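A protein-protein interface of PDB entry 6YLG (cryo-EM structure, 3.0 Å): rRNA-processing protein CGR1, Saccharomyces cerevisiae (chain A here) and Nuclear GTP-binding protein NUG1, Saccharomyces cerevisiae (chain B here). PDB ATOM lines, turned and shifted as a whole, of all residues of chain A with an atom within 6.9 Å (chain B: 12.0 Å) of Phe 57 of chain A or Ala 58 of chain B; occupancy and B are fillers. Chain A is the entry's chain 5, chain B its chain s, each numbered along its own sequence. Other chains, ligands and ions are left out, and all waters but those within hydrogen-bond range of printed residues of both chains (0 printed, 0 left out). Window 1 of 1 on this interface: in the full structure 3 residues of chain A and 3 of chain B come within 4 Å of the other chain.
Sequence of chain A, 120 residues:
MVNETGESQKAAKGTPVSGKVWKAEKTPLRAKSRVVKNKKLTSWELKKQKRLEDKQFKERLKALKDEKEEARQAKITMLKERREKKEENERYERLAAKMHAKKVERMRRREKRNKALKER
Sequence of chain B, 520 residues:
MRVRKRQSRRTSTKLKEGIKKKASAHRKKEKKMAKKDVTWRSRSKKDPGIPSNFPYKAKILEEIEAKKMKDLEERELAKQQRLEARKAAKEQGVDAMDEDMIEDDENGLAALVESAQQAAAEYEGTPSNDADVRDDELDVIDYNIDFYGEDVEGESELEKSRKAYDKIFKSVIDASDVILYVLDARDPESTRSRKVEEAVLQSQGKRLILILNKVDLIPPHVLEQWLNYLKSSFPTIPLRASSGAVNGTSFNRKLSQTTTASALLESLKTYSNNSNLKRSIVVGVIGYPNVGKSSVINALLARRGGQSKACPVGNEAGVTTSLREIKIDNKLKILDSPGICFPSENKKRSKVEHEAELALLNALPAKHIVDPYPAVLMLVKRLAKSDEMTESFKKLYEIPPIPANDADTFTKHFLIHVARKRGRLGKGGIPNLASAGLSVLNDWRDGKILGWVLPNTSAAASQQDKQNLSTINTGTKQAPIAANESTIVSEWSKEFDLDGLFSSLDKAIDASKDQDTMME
Among the printed residues, merely in contact across the chains: Phe 57 of chain A with Lys 57 of chain B (3.3 Å), Phe 57 of chain A with Ala 58 of chain B (3.97 Å), Phe 57 of chain A with Leu 61 of chain B (3.3 Å) and Arg 60 of chain A with Leu 61 of chain B (3.3 Å).
Glu 53 of chain A touches none of the printed residues of chain B. Asp 54 of chain A touches just one residue of chain B: Lys 57. Of chain B, only Lys 57, Ala 58 and Leu 61 come within 4 Å of Phe 57 of chain A. Glu 59 of chain A touches none of the printed residues of chain B. No residue of chain B comes within 4 Å of Leu 61 of chain A. Of the printed residues of chain A, Lys 57 of chain B touches Asp 54 (2.6 Å) and Phe 57 (3.3 Å). Of chain A, only Phe 57 (3.97 Å) and Arg 60 (3.3 Å) come within 4 Å of Ala 58 of chain B. Of the printed residues of chain A, Leu 61 of chain B touches Phe 57 (3.3 Å) and Arg 60 (3.3 Å). The nearest residue of chain A that does not touch Ala 58 of chain B is Glu 53 of chain A (6.4 Å).
The side-chain carboxylate (OD1) of Asp 54 of chain A lies within salt-bridge range of the side-chain amino group (NZ) of Lys 57 of chain B (2.6 Å). The backbone carbonyl oxygen (O) of Ala 58 of chain B lies within hydrogen-bond range of the guanidinium group (NH2) of Arg 60 of chain A.
Hydrophobic or aromatic side chains of chain B within 4 Å of the printed part of chain A: Leu 61. Printed residues of chain A that touch a printed residue of chain B: Asp 54, Phe 57 and Arg 60. Hydrophobic or aromatic side chains of chain A within 4 Å of the printed part of chain B: Phe 57. Among the printed residues, 6 pairs touch across the chains. Among the printed residues, Asp or Glu carboxylates within 4 Å of a Lys or Arg side-chain nitrogen of the other chain: Asp 54 of chain A with Lys 57 of chain B.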
ATOM      1  N   LEU A  52      15.455  24.309  -5.838  1.00  0.00           N
ATOM      2  CA  LEU A  52      14.586  23.156  -6.032  1.00  0.00           C
ATOM      3  C   LEU A  52      15.395  21.869  -6.146  1.00  0.00           C
ATOM      4  O   LEU A  52      14.995  20.822  -5.620  1.00  0.00           O
ATOM      5  CB  LEU A  52      13.728  23.371  -7.276  1.00  0.00           C
ATOM      6  CG  LEU A  52      12.606  22.367  -7.533  1.00  0.00           C
ATOM      7  CD1 LEU A  52      11.498  22.523  -6.504  1.00  0.00           C
ATOM      8  CD2 LEU A  52      12.074  22.558  -8.940  1.00  0.00           C
ATOM      9  N   GLU A  53      16.537  21.922  -6.830  1.00  0.00           N
ATOM     10  CA  GLU A  53      17.362  20.723  -6.938  1.00  0.00           C
ATOM     11  C   GLU A  53      17.996  20.373  -5.596  1.00  0.00           C
ATOM     12  O   GLU A  53      18.179  19.189  -5.283  1.00  0.00           O
ATOM     13  CB  GLU A  53      18.414  20.901  -8.043  1.00  0.00           C
ATOM     14  CG  GLU A  53      19.793  21.403  -7.621  1.00  0.00           C
ATOM     15  CD  GLU A  53      20.713  21.624  -8.807  1.00  0.00           C
ATOM     16  OE1 GLU A  53      20.238  21.527  -9.958  1.00  0.00           O
ATOM     17  OE2 GLU A  53      21.913  21.896  -8.591  1.00  0.00           O
ATOM     18  N   ASP A  54      18.321  21.384  -4.784  1.00  0.00           N
ATOM     19  CA  ASP A  54      18.712  21.174  -3.393  1.00  0.00           C
ATOM     20  C   ASP A  54      17.646  20.385  -2.643  1.00  0.00           C
ATOM     21  O   ASP A  54      17.964  19.460  -1.883  1.00  0.00           O
ATOM     22  CB  ASP A  54      18.944  22.523  -2.702  1.00  0.00           C
ATOM     23  CG  ASP A  54      20.405  22.971  -2.724  1.00  0.00           C
ATOM     24  OD1 ASP A  54      21.319  22.131  -2.855  1.00  0.00           O
ATOM     25  OD2 ASP A  54      20.637  24.193  -2.602  1.00  0.00           O
ATOM     26  N   LYS A  55      16.395  20.826  -2.796  1.00  0.00           N
ATOM     27  CA  LYS A  55      15.284  20.142  -2.140  1.00  0.00           C
ATOM     28  C   LYS A  55      15.161  18.699  -2.619  1.00  0.00           C
ATOM     29  O   LYS A  55      14.903  17.791  -1.819  1.00  0.00           O
ATOM     30  CB  LYS A  55      13.982  20.898  -2.394  1.00  0.00           C
ATOM     31  CG  LYS A  55      13.910  22.247  -1.701  1.00  0.00           C
ATOM     32  CD  LYS A  55      12.612  22.975  -2.020  1.00  0.00           C
ATOM     33  CE  LYS A  55      11.570  22.795  -0.927  1.00  0.00           C
ATOM     34  NZ  LYS A  55      11.686  23.845   0.122  1.00  0.00           N
ATOM     35  N   GLN A  56      15.330  18.474  -3.922  1.00  0.00           N
ATOM     36  CA  GLN A  56      15.279  17.117  -4.465  1.00  0.00           C
ATOM     37  C   GLN A  56      16.349  16.234  -3.830  1.00  0.00           C
ATOM     38  O   GLN A  56      16.081  15.093  -3.424  1.00  0.00           O
ATOM     39  CB  GLN A  56      15.462  17.148  -5.987  1.00  0.00           C
ATOM     40  CG  GLN A  56      14.184  16.997  -6.807  1.00  0.00           C
ATOM     41  CD  GLN A  56      13.521  18.328  -7.102  1.00  0.00           C
ATOM     42  OE1 GLN A  56      14.149  19.238  -7.645  1.00  0.00           O
ATOM     43  NE2 GLN A  56      12.246  18.446  -6.753  1.00  0.00           N
ATOM     44  N   PHE A  57      17.579  16.749  -3.756  1.00  0.00           N
ATOM     45  CA  PHE A  57      18.668  15.991  -3.147  1.00  0.00           C
ATOM     46  C   PHE A  57      18.370  15.675  -1.686  1.00  0.00           C
ATOM     47  O   PHE A  57      18.613  14.554  -1.223  1.00  0.00           O
ATOM     48  CB  PHE A  57      19.976  16.771  -3.263  1.00  0.00           C
ATOM     49  CG  PHE A  57      21.163  16.046  -2.699  1.00  0.00           C
ATOM     50  CD1 PHE A  57      21.803  15.065  -3.433  1.00  0.00           C
ATOM     51  CD2 PHE A  57      21.634  16.339  -1.431  1.00  0.00           C
ATOM     52  CE1 PHE A  57      22.893  14.395  -2.919  1.00  0.00           C
ATOM     53  CE2 PHE A  57      22.723  15.672  -0.911  1.00  0.00           C
ATOM     54  CZ  PHE A  57      23.353  14.699  -1.653  1.00  0.00           C
ATOM     55  N   LYS A  58      17.860  16.661  -0.944  1.00  0.00           N
ATOM     56  CA  LYS A  58      17.528  16.441   0.461  1.00  0.00           C
ATOM     57  C   LYS A  58      16.463  15.362   0.610  1.00  0.00           C
ATOM     58  O   LYS A  58      16.555  14.503   1.498  1.00  0.00           O
ATOM     59  CB  LYS A  58      17.053  17.748   1.090  1.00  0.00           C
ATOM     60  CG  LYS A  58      18.157  18.781   1.264  1.00  0.00           C
ATOM     61  CD  LYS A  58      17.612  20.164   1.615  1.00  0.00           C
ATOM     62  CE  LYS A  58      17.493  20.371   3.118  1.00  0.00           C
ATOM     63  NZ  LYS A  58      17.181  21.784   3.468  1.00  0.00           N
ATOM     64  N   GLU A  59      15.448  15.388  -0.256  1.00  0.00           N
ATOM     65  CA  GLU A  59      14.402  14.374  -0.204  1.00  0.00           C
ATOM     66  C   GLU A  59      14.971  12.984  -0.454  1.00  0.00           C
ATOM     67  O   GLU A  59      14.661  12.038   0.282  1.00  0.00           O
ATOM     68  CB  GLU A  59      13.313  14.697  -1.225  1.00  0.00           C
ATOM     69  CG  GLU A  59      12.426  15.871  -0.838  1.00  0.00           C
ATOM     70  CD  GLU A  59      11.407  16.212  -1.911  1.00  0.00           C
ATOM     71  OE1 GLU A  59      11.671  15.923  -3.097  1.00  0.00           O
ATOM     72  OE2 GLU A  59      10.343  16.769  -1.571  1.00  0.00           O
ATOM     73  N   ARG A  60      15.812  12.840  -1.483  1.00  0.00           N
ATOM     74  CA  ARG A  60      16.377  11.525  -1.781  1.00  0.00           C
ATOM     75  C   ARG A  60      17.259  11.029  -0.641  1.00  0.00           C
ATOM     76  O   ARG A  60      17.214   9.847  -0.276  1.00  0.00           O
ATOM     77  CB  ARG A  60      17.181  11.578  -3.078  1.00  0.00           C
ATOM     78  CG  ARG A  60      16.366  11.280  -4.319  1.00  0.00           C
ATOM     79  CD  ARG A  60      16.978  11.926  -5.544  1.00  0.00           C
ATOM     80  NE  ARG A  60      18.282  11.350  -5.867  1.00  0.00           N
ATOM     81  CZ  ARG A  60      19.189  11.915  -6.662  1.00  0.00           C
ATOM     82  NH1 ARG A  60      18.963  13.090  -7.240  1.00  0.00           N
ATOM     83  NH2 ARG A  60      20.340  11.296  -6.884  1.00  0.00           N
ATOM     84  N   LEU A  61      18.058  11.926  -0.064  1.00  0.00           N
ATOM     85  CA  LEU A  61      18.944  11.544   1.029  1.00  0.00           C
ATOM     86  C   LEU A  61      18.156  11.084   2.250  1.00  0.00           C
ATOM     87  O   LEU A  61      18.477  10.050   2.864  1.00  0.00           O
ATOM     88  CB  LEU A  61      19.839  12.730   1.373  1.00  0.00           C
ATOM     89  CG  LEU A  61      21.076  12.498   2.237  1.00  0.00           C
ATOM     90  CD1 LEU A  61      22.046  11.535   1.567  1.00  0.00           C
ATOM     91  CD2 LEU A  61      21.755  13.830   2.512  1.00  0.00           C
ATOM     92  N   LYS A  62      17.130  11.851   2.630  1.00  0.00           N
ATOM     93  CA  LYS A  62      16.314  11.466   3.773  1.00  0.00           C
ATOM     94  C   LYS A  62      15.554  10.186   3.490  1.00  0.00           C
ATOM     95  O   LYS A  62      15.287   9.408   4.412  1.00  0.00           O
ATOM     96  CB  LYS A  62      15.346  12.585   4.136  1.00  0.00           C
ATOM     97  CG  LYS A  62      14.451  12.253   5.311  1.00  0.00           C
ATOM     98  CD  LYS A  62      13.915  13.501   5.988  1.00  0.00           C
ATOM     99  CE  LYS A  62      13.029  14.330   5.063  1.00  0.00           C
ATOM    100  NZ  LYS A  62      11.885  13.563   4.494  1.00  0.00           N
ATOM    101  N   ALA A  63      15.196   9.948   2.230  1.00  0.00           N
ATOM    102  CA  ALA A  63      14.593   8.670   1.880  1.00  0.00           C
ATOM    103  C   ALA A  63      15.562   7.525   2.145  1.00  0.00           C
ATOM    104  O   ALA A  63      15.206   6.550   2.812  1.00  0.00           O
ATOM    105  CB  ALA A  63      14.136   8.689   0.419  1.00  0.00           C
ATOM    106  N   ASP B  47      30.228   9.517  10.135  1.00  0.00           N
ATOM    107  CA  ASP B  47      30.808  10.155   8.965  1.00  0.00           C
ATOM    108  C   ASP B  47      30.009  11.413   8.635  1.00  0.00           C
ATOM    109  O   ASP B  47      28.774  11.364   8.628  1.00  0.00           O
ATOM    110  CB  ASP B  47      30.817   9.192   7.785  1.00  0.00           C
ATOM    111  CG  ASP B  47      31.583   9.722   6.589  1.00  0.00           C
ATOM    112  OD1 ASP B  47      32.828   9.585   6.569  1.00  0.00           O
ATOM    113  OD2 ASP B  47      30.951  10.294   5.673  1.00  0.00           O
ATOM    114  N   PRO B  48      30.656  12.556   8.370  1.00  0.00           N
ATOM    115  CA  PRO B  48      29.895  13.809   8.297  1.00  0.00           C
ATOM    116  C   PRO B  48      28.973  13.904   7.093  1.00  0.00           C
ATOM    117  O   PRO B  48      28.041  14.718   7.121  1.00  0.00           O
ATOM    118  CB  PRO B  48      30.988  14.881   8.250  1.00  0.00           C
ATOM    119  CG  PRO B  48      32.148  14.211   7.660  1.00  0.00           C
ATOM    120  CD  PRO B  48      32.079  12.771   8.054  1.00  0.00           C
ATOM    121  N   GLY B  49      29.208  13.121   6.042  1.00  0.00           N
ATOM    122  CA  GLY B  49      28.274  13.009   4.937  1.00  0.00           C
ATOM    123  C   GLY B  49      28.780  13.633   3.654  1.00  0.00           C
ATOM    124  O   GLY B  49      29.980  13.754   3.393  1.00  0.00           O
ATOM    125  N   ILE B  50      27.810  14.015   2.829  1.00  0.00           N
ATOM    126  CA  ILE B  50      28.035  14.619   1.518  1.00  0.00           C
ATOM    127  C   ILE B  50      27.820  16.123   1.670  1.00  0.00           C
ATOM    128  O   ILE B  50      26.678  16.588   1.544  1.00  0.00           O
ATOM    129  CB  ILE B  50      27.086  14.012   0.468  1.00  0.00           C
ATOM    130  CG1 ILE B  50      27.042  12.478   0.575  1.00  0.00           C
ATOM    131  CG2 ILE B  50      27.471  14.429  -0.948  1.00  0.00           C
ATOM    132  CD1 ILE B  50      28.399  11.791   0.677  1.00  0.00           C
ATOM    133  N   PRO B  51      28.852  16.924   1.943  1.00  0.00           N
ATOM    134  CA  PRO B  51      28.605  18.322   2.311  1.00  0.00           C
ATOM    135  C   PRO B  51      28.094  19.173   1.160  1.00  0.00           C
ATOM    136  O   PRO B  51      28.441  18.975  -0.006  1.00  0.00           O
ATOM    137  CB  PRO B  51      29.979  18.811   2.786  1.00  0.00           C
ATOM    138  CG  PRO B  51      30.935  17.948   2.100  1.00  0.00           C
ATOM    139  CD  PRO B  51      30.287  16.602   2.047  1.00  0.00           C
ATOM    140  N   SER B  52      27.256  20.142   1.521  1.00  0.00           N
ATOM    141  CA  SER B  52      26.649  21.045   0.560  1.00  0.00           C
ATOM    142  C   SER B  52      27.697  22.000  -0.011  1.00  0.00           C
ATOM    143  O   SER B  52      28.861  22.013   0.399  1.00  0.00           O
ATOM    144  CB  SER B  52      25.503  21.814   1.212  1.00  0.00           C
ATOM    145  OG  SER B  52      24.495  20.929   1.664  1.00  0.00           O
ATOM    146  N   ASN B  53      27.259  22.785  -1.004  1.00  0.00           N
ATOM    147  CA  ASN B  53      28.078  23.660  -1.846  1.00  0.00           C
ATOM    148  C   ASN B  53      28.895  22.880  -2.875  1.00  0.00           C
ATOM    149  O   ASN B  53      29.536  23.483  -3.740  1.00  0.00           O
ATOM    150  CB  ASN B  53      29.016  24.540  -1.012  1.00  0.00           C
ATOM    151  CG  ASN B  53      28.307  25.234   0.132  1.00  0.00           C
ATOM    152  OD1 ASN B  53      28.644  25.034   1.298  1.00  0.00           O
ATOM    153  ND2 ASN B  53      27.326  26.065  -0.199  1.00  0.00           N
ATOM    154  N   PHE B  54      28.866  21.551  -2.809  1.00  0.00           N
ATOM    155  CA  PHE B  54      29.479  20.715  -3.826  1.00  0.00           C
ATOM    156  C   PHE B  54      28.489  20.548  -4.974  1.00  0.00           C
ATOM    157  O   PHE B  54      27.436  19.932  -4.776  1.00  0.00           O
ATOM    158  CB  PHE B  54      29.839  19.368  -3.225  1.00  0.00           C
ATOM    159  CG  PHE B  54      30.693  18.508  -4.106  1.00  0.00           C
ATOM    160  CD1 PHE B  54      32.038  18.778  -4.268  1.00  0.00           C
ATOM    161  CD2 PHE B  54      30.155  17.413  -4.752  1.00  0.00           C
ATOM    162  CE1 PHE B  54      32.823  17.983  -5.070  1.00  0.00           C
ATOM    163  CE2 PHE B  54      30.936  16.614  -5.553  1.00  0.00           C
ATOM    164  CZ  PHE B  54      32.271  16.899  -5.712  1.00  0.00           C
ATOM    165  N   PRO B  55      28.767  21.080  -6.178  1.00  0.00           N
ATOM    166  CA  PRO B  55      27.700  21.170  -7.183  1.00  0.00           C
ATOM    167  C   PRO B  55      27.242  19.816  -7.701  1.00  0.00           C
ATOM    168  O   PRO B  55      26.043  19.593  -7.892  1.00  0.00           O
ATOM    169  CB  PRO B  55      28.347  22.003  -8.293  1.00  0.00           C
ATOM    170  CG  PRO B  55      29.775  21.653  -8.209  1.00  0.00           C
ATOM    171  CD  PRO B  55      30.065  21.493  -6.746  1.00  0.00           C
ATOM    172  N   TYR B  56      28.187  18.912  -7.931  1.00  0.00           N
ATOM    173  CA  TYR B  56      27.892  17.575  -8.448  1.00  0.00           C
ATOM    174  C   TYR B  56      27.741  16.569  -7.314  1.00  0.00           C
ATOM    175  O   TYR B  56      28.372  15.512  -7.303  1.00  0.00           O
ATOM    176  CB  TYR B  56      28.981  17.143  -9.426  1.00  0.00           C
ATOM    177  CG  TYR B  56      29.271  18.147 -10.533  1.00  0.00           C
ATOM    178  CD1 TYR B  56      28.272  18.970 -11.045  1.00  0.00           C
ATOM    179  CD2 TYR B  56      30.548  18.274 -11.062  1.00  0.00           C
ATOM    180  CE1 TYR B  56      28.538  19.884 -12.045  1.00  0.00           C
ATOM    181  CE2 TYR B  56      30.822  19.185 -12.064  1.00  0.00           C
ATOM    182  CZ  TYR B  56      29.814  19.988 -12.552  1.00  0.00           C
ATOM    183  OH  TYR B  56      30.083  20.896 -13.549  1.00  0.00           O
ATOM    184  N   LYS B  57      26.884  16.896  -6.342  1.00  0.00           N
ATOM    185  CA  LYS B  57      26.596  15.989  -5.238  1.00  0.00           C
ATOM    186  C   LYS B  57      25.500  14.986  -5.572  1.00  0.00           C
ATOM    187  O   LYS B  57      25.432  13.931  -4.932  1.00  0.00           O
ATOM    188  CB  LYS B  57      26.191  16.779  -3.992  1.00  0.00           C
ATOM    189  CG  LYS B  57      24.850  17.484  -4.101  1.00  0.00           C
ATOM    190  CD  LYS B  57      24.747  18.621  -3.099  1.00  0.00           C
ATOM    191  CE  LYS B  57      23.364  19.243  -3.103  1.00  0.00           C
ATOM    192  NZ  LYS B  57      23.367  20.588  -2.479  1.00  0.00           N
ATOM    193  N   ALA B  58      24.649  15.286  -6.550  1.00  0.00           N
ATOM    194  CA  ALA B  58      23.559  14.396  -6.929  1.00  0.00           C
ATOM    195  C   ALA B  58      24.018  13.182  -7.728  1.00  0.00           C
ATOM    196  O   ALA B  58      23.174  12.357  -8.096  1.00  0.00           O
ATOM    197  CB  ALA B  58      22.517  15.173  -7.734  1.00  0.00           C
ATOM    198  N   LYS B  59      25.319  13.047  -7.999  1.00  0.00           N
ATOM    199  CA  LYS B  59      25.855  11.903  -8.723  1.00  0.00           C
ATOM    200  C   LYS B  59      26.411  10.825  -7.807  1.00  0.00           C
ATOM    201  O   LYS B  59      26.489   9.664  -8.222  1.00  0.00           O
ATOM    202  CB  LYS B  59      26.969  12.355  -9.673  1.00  0.00           C
ATOM    203  CG  LYS B  59      26.500  13.208 -10.838  1.00  0.00           C
ATOM    204  CD  LYS B  59      27.685  13.639 -11.685  1.00  0.00           C
ATOM    205  CE  LYS B  59      27.283  14.028 -13.095  1.00  0.00           C
ATOM    206  NZ  LYS B  59      28.463  14.074 -13.994  1.00  0.00           N
ATOM    207  N   ILE B  60      26.791  11.179  -6.577  1.00  0.00           N
ATOM    208  CA  ILE B  60      27.313  10.187  -5.644  1.00  0.00           C
ATOM    209  C   ILE B  60      26.196   9.275  -5.147  1.00  0.00           C
ATOM    210  O   ILE B  60      26.459   8.170  -4.658  1.00  0.00           O
ATOM    211  CB  ILE B  60      28.049  10.894  -4.487  1.00  0.00           C
ATOM    212  CG1 ILE B  60      29.233  11.702  -5.038  1.00  0.00           C
ATOM    213  CG2 ILE B  60      28.520   9.883  -3.429  1.00  0.00           C
ATOM    214  CD1 ILE B  60      28.963  13.181  -5.190  1.00  0.00           C
ATOM    215  N   LEU B  61      24.938   9.701  -5.276  1.00  0.00           N
ATOM    216  CA  LEU B  61      23.787   8.887  -4.898  1.00  0.00           C
ATOM    217  C   LEU B  61      23.489   7.763  -5.891  1.00  0.00           C
ATOM    218  O   LEU B  61      22.524   7.025  -5.639  1.00  0.00           O
ATOM    219  CB  LEU B  61      22.553   9.783  -4.769  1.00  0.00           C
ATOM    220  CG  LEU B  61      22.499  10.810  -3.635  1.00  0.00           C
ATOM    221  CD1 LEU B  61      21.216  11.627  -3.752  1.00  0.00           C
ATOM    222  CD2 LEU B  61      22.596  10.149  -2.267  1.00  0.00           C
ATOM    223  N   GLU B  62      24.270   7.598  -6.963  1.00  0.00           N
ATOM    224  CA  GLU B  62      23.908   6.736  -8.078  1.00  0.00           C
ATOM    225  C   GLU B  62      24.836   5.548  -8.280  1.00  0.00           C
ATOM    226  O   GLU B  62      24.482   4.642  -9.042  1.00  0.00           O
ATOM    227  CB  GLU B  62      23.860   7.552  -9.380  1.00  0.00           C
ATOM    228  CG  GLU B  62      22.976   8.791  -9.299  1.00  0.00           C
ATOM    229  CD  GLU B  62      22.935   9.566 -10.601  1.00  0.00           C
ATOM    230  OE1 GLU B  62      23.549   9.105 -11.586  1.00  0.00           O
ATOM    231  OE2 GLU B  62      22.291  10.635 -10.639  1.00  0.00           O
ATOM    232  N   GLU B  63      25.997   5.516  -7.628  1.00  0.00           N
ATOM    233  CA  GLU B  63      26.911   4.380  -7.717  1.00  0.00           C
ATOM    234  C   GLU B  63      26.572   3.273  -6.724  1.00  0.00           C
ATOM    235  O   GLU B  63      27.372   2.347  -6.553  1.00  0.00           O
ATOM    236  CB  GLU B  63      28.359   4.836  -7.488  1.00  0.00           C
ATOM    237  CG  GLU B  63      28.941   5.731  -8.585  1.00  0.00           C
ATOM    238  CD  GLU B  63      28.430   7.157  -8.532  1.00  0.00           C
ATOM    239  OE1 GLU B  63      27.961   7.579  -7.458  1.00  0.00           O
ATOM    240  OE2 GLU B  63      28.497   7.856  -9.565  1.00  0.00           O
ATOM    241  N   ILE B  64      25.407   3.336  -6.081  1.00  0.00           N
ATOM    242  CA  ILE B  64      25.123   2.444  -4.962  1.00  0.00           C
ATOM    243  C   ILE B  64      24.706   1.068  -5.464  1.00  0.00           C
ATOM    244  O   ILE B  64      25.311   0.051  -5.107  1.00  0.00           O
ATOM    245  CB  ILE B  64      24.044   3.059  -4.047  1.00  0.00           C
ATOM    246  CG1 ILE B  64      24.284   4.562  -3.814  1.00  0.00           C
ATOM    247  CG2 ILE B  64      23.986   2.314  -2.713  1.00  0.00           C
ATOM    248  CD1 ILE B  64      25.711   4.941  -3.449  1.00  0.00           C
ATOM    249  N   GLU B  65      23.670   1.012  -6.294  1.00  0.00           N
ATOM    250  CA  GLU B  65      23.152  -0.259  -6.779  1.00  0.00           C
ATOM    251  C   GLU B  65      24.072  -0.841  -7.846  1.00  0.00           C
ATOM    252  O   GLU B  65      25.254  -1.077  -7.596  1.00  0.00           O
ATOM    253  CB  GLU B  65      21.737  -0.079  -7.336  1.00  0.00           C
ATOM    254  CG  GLU B  65      20.830  -1.305  -7.183  1.00  0.00           C
ATOM    255  CD  GLU B  65      21.059  -2.370  -8.241  1.00  0.00           C
ATOM    256  OE1 GLU B  65      21.734  -2.093  -9.256  1.00  0.00           O
ATOM    257  OE2 GLU B  65      20.558  -3.499  -8.054  1.00  0.00           O
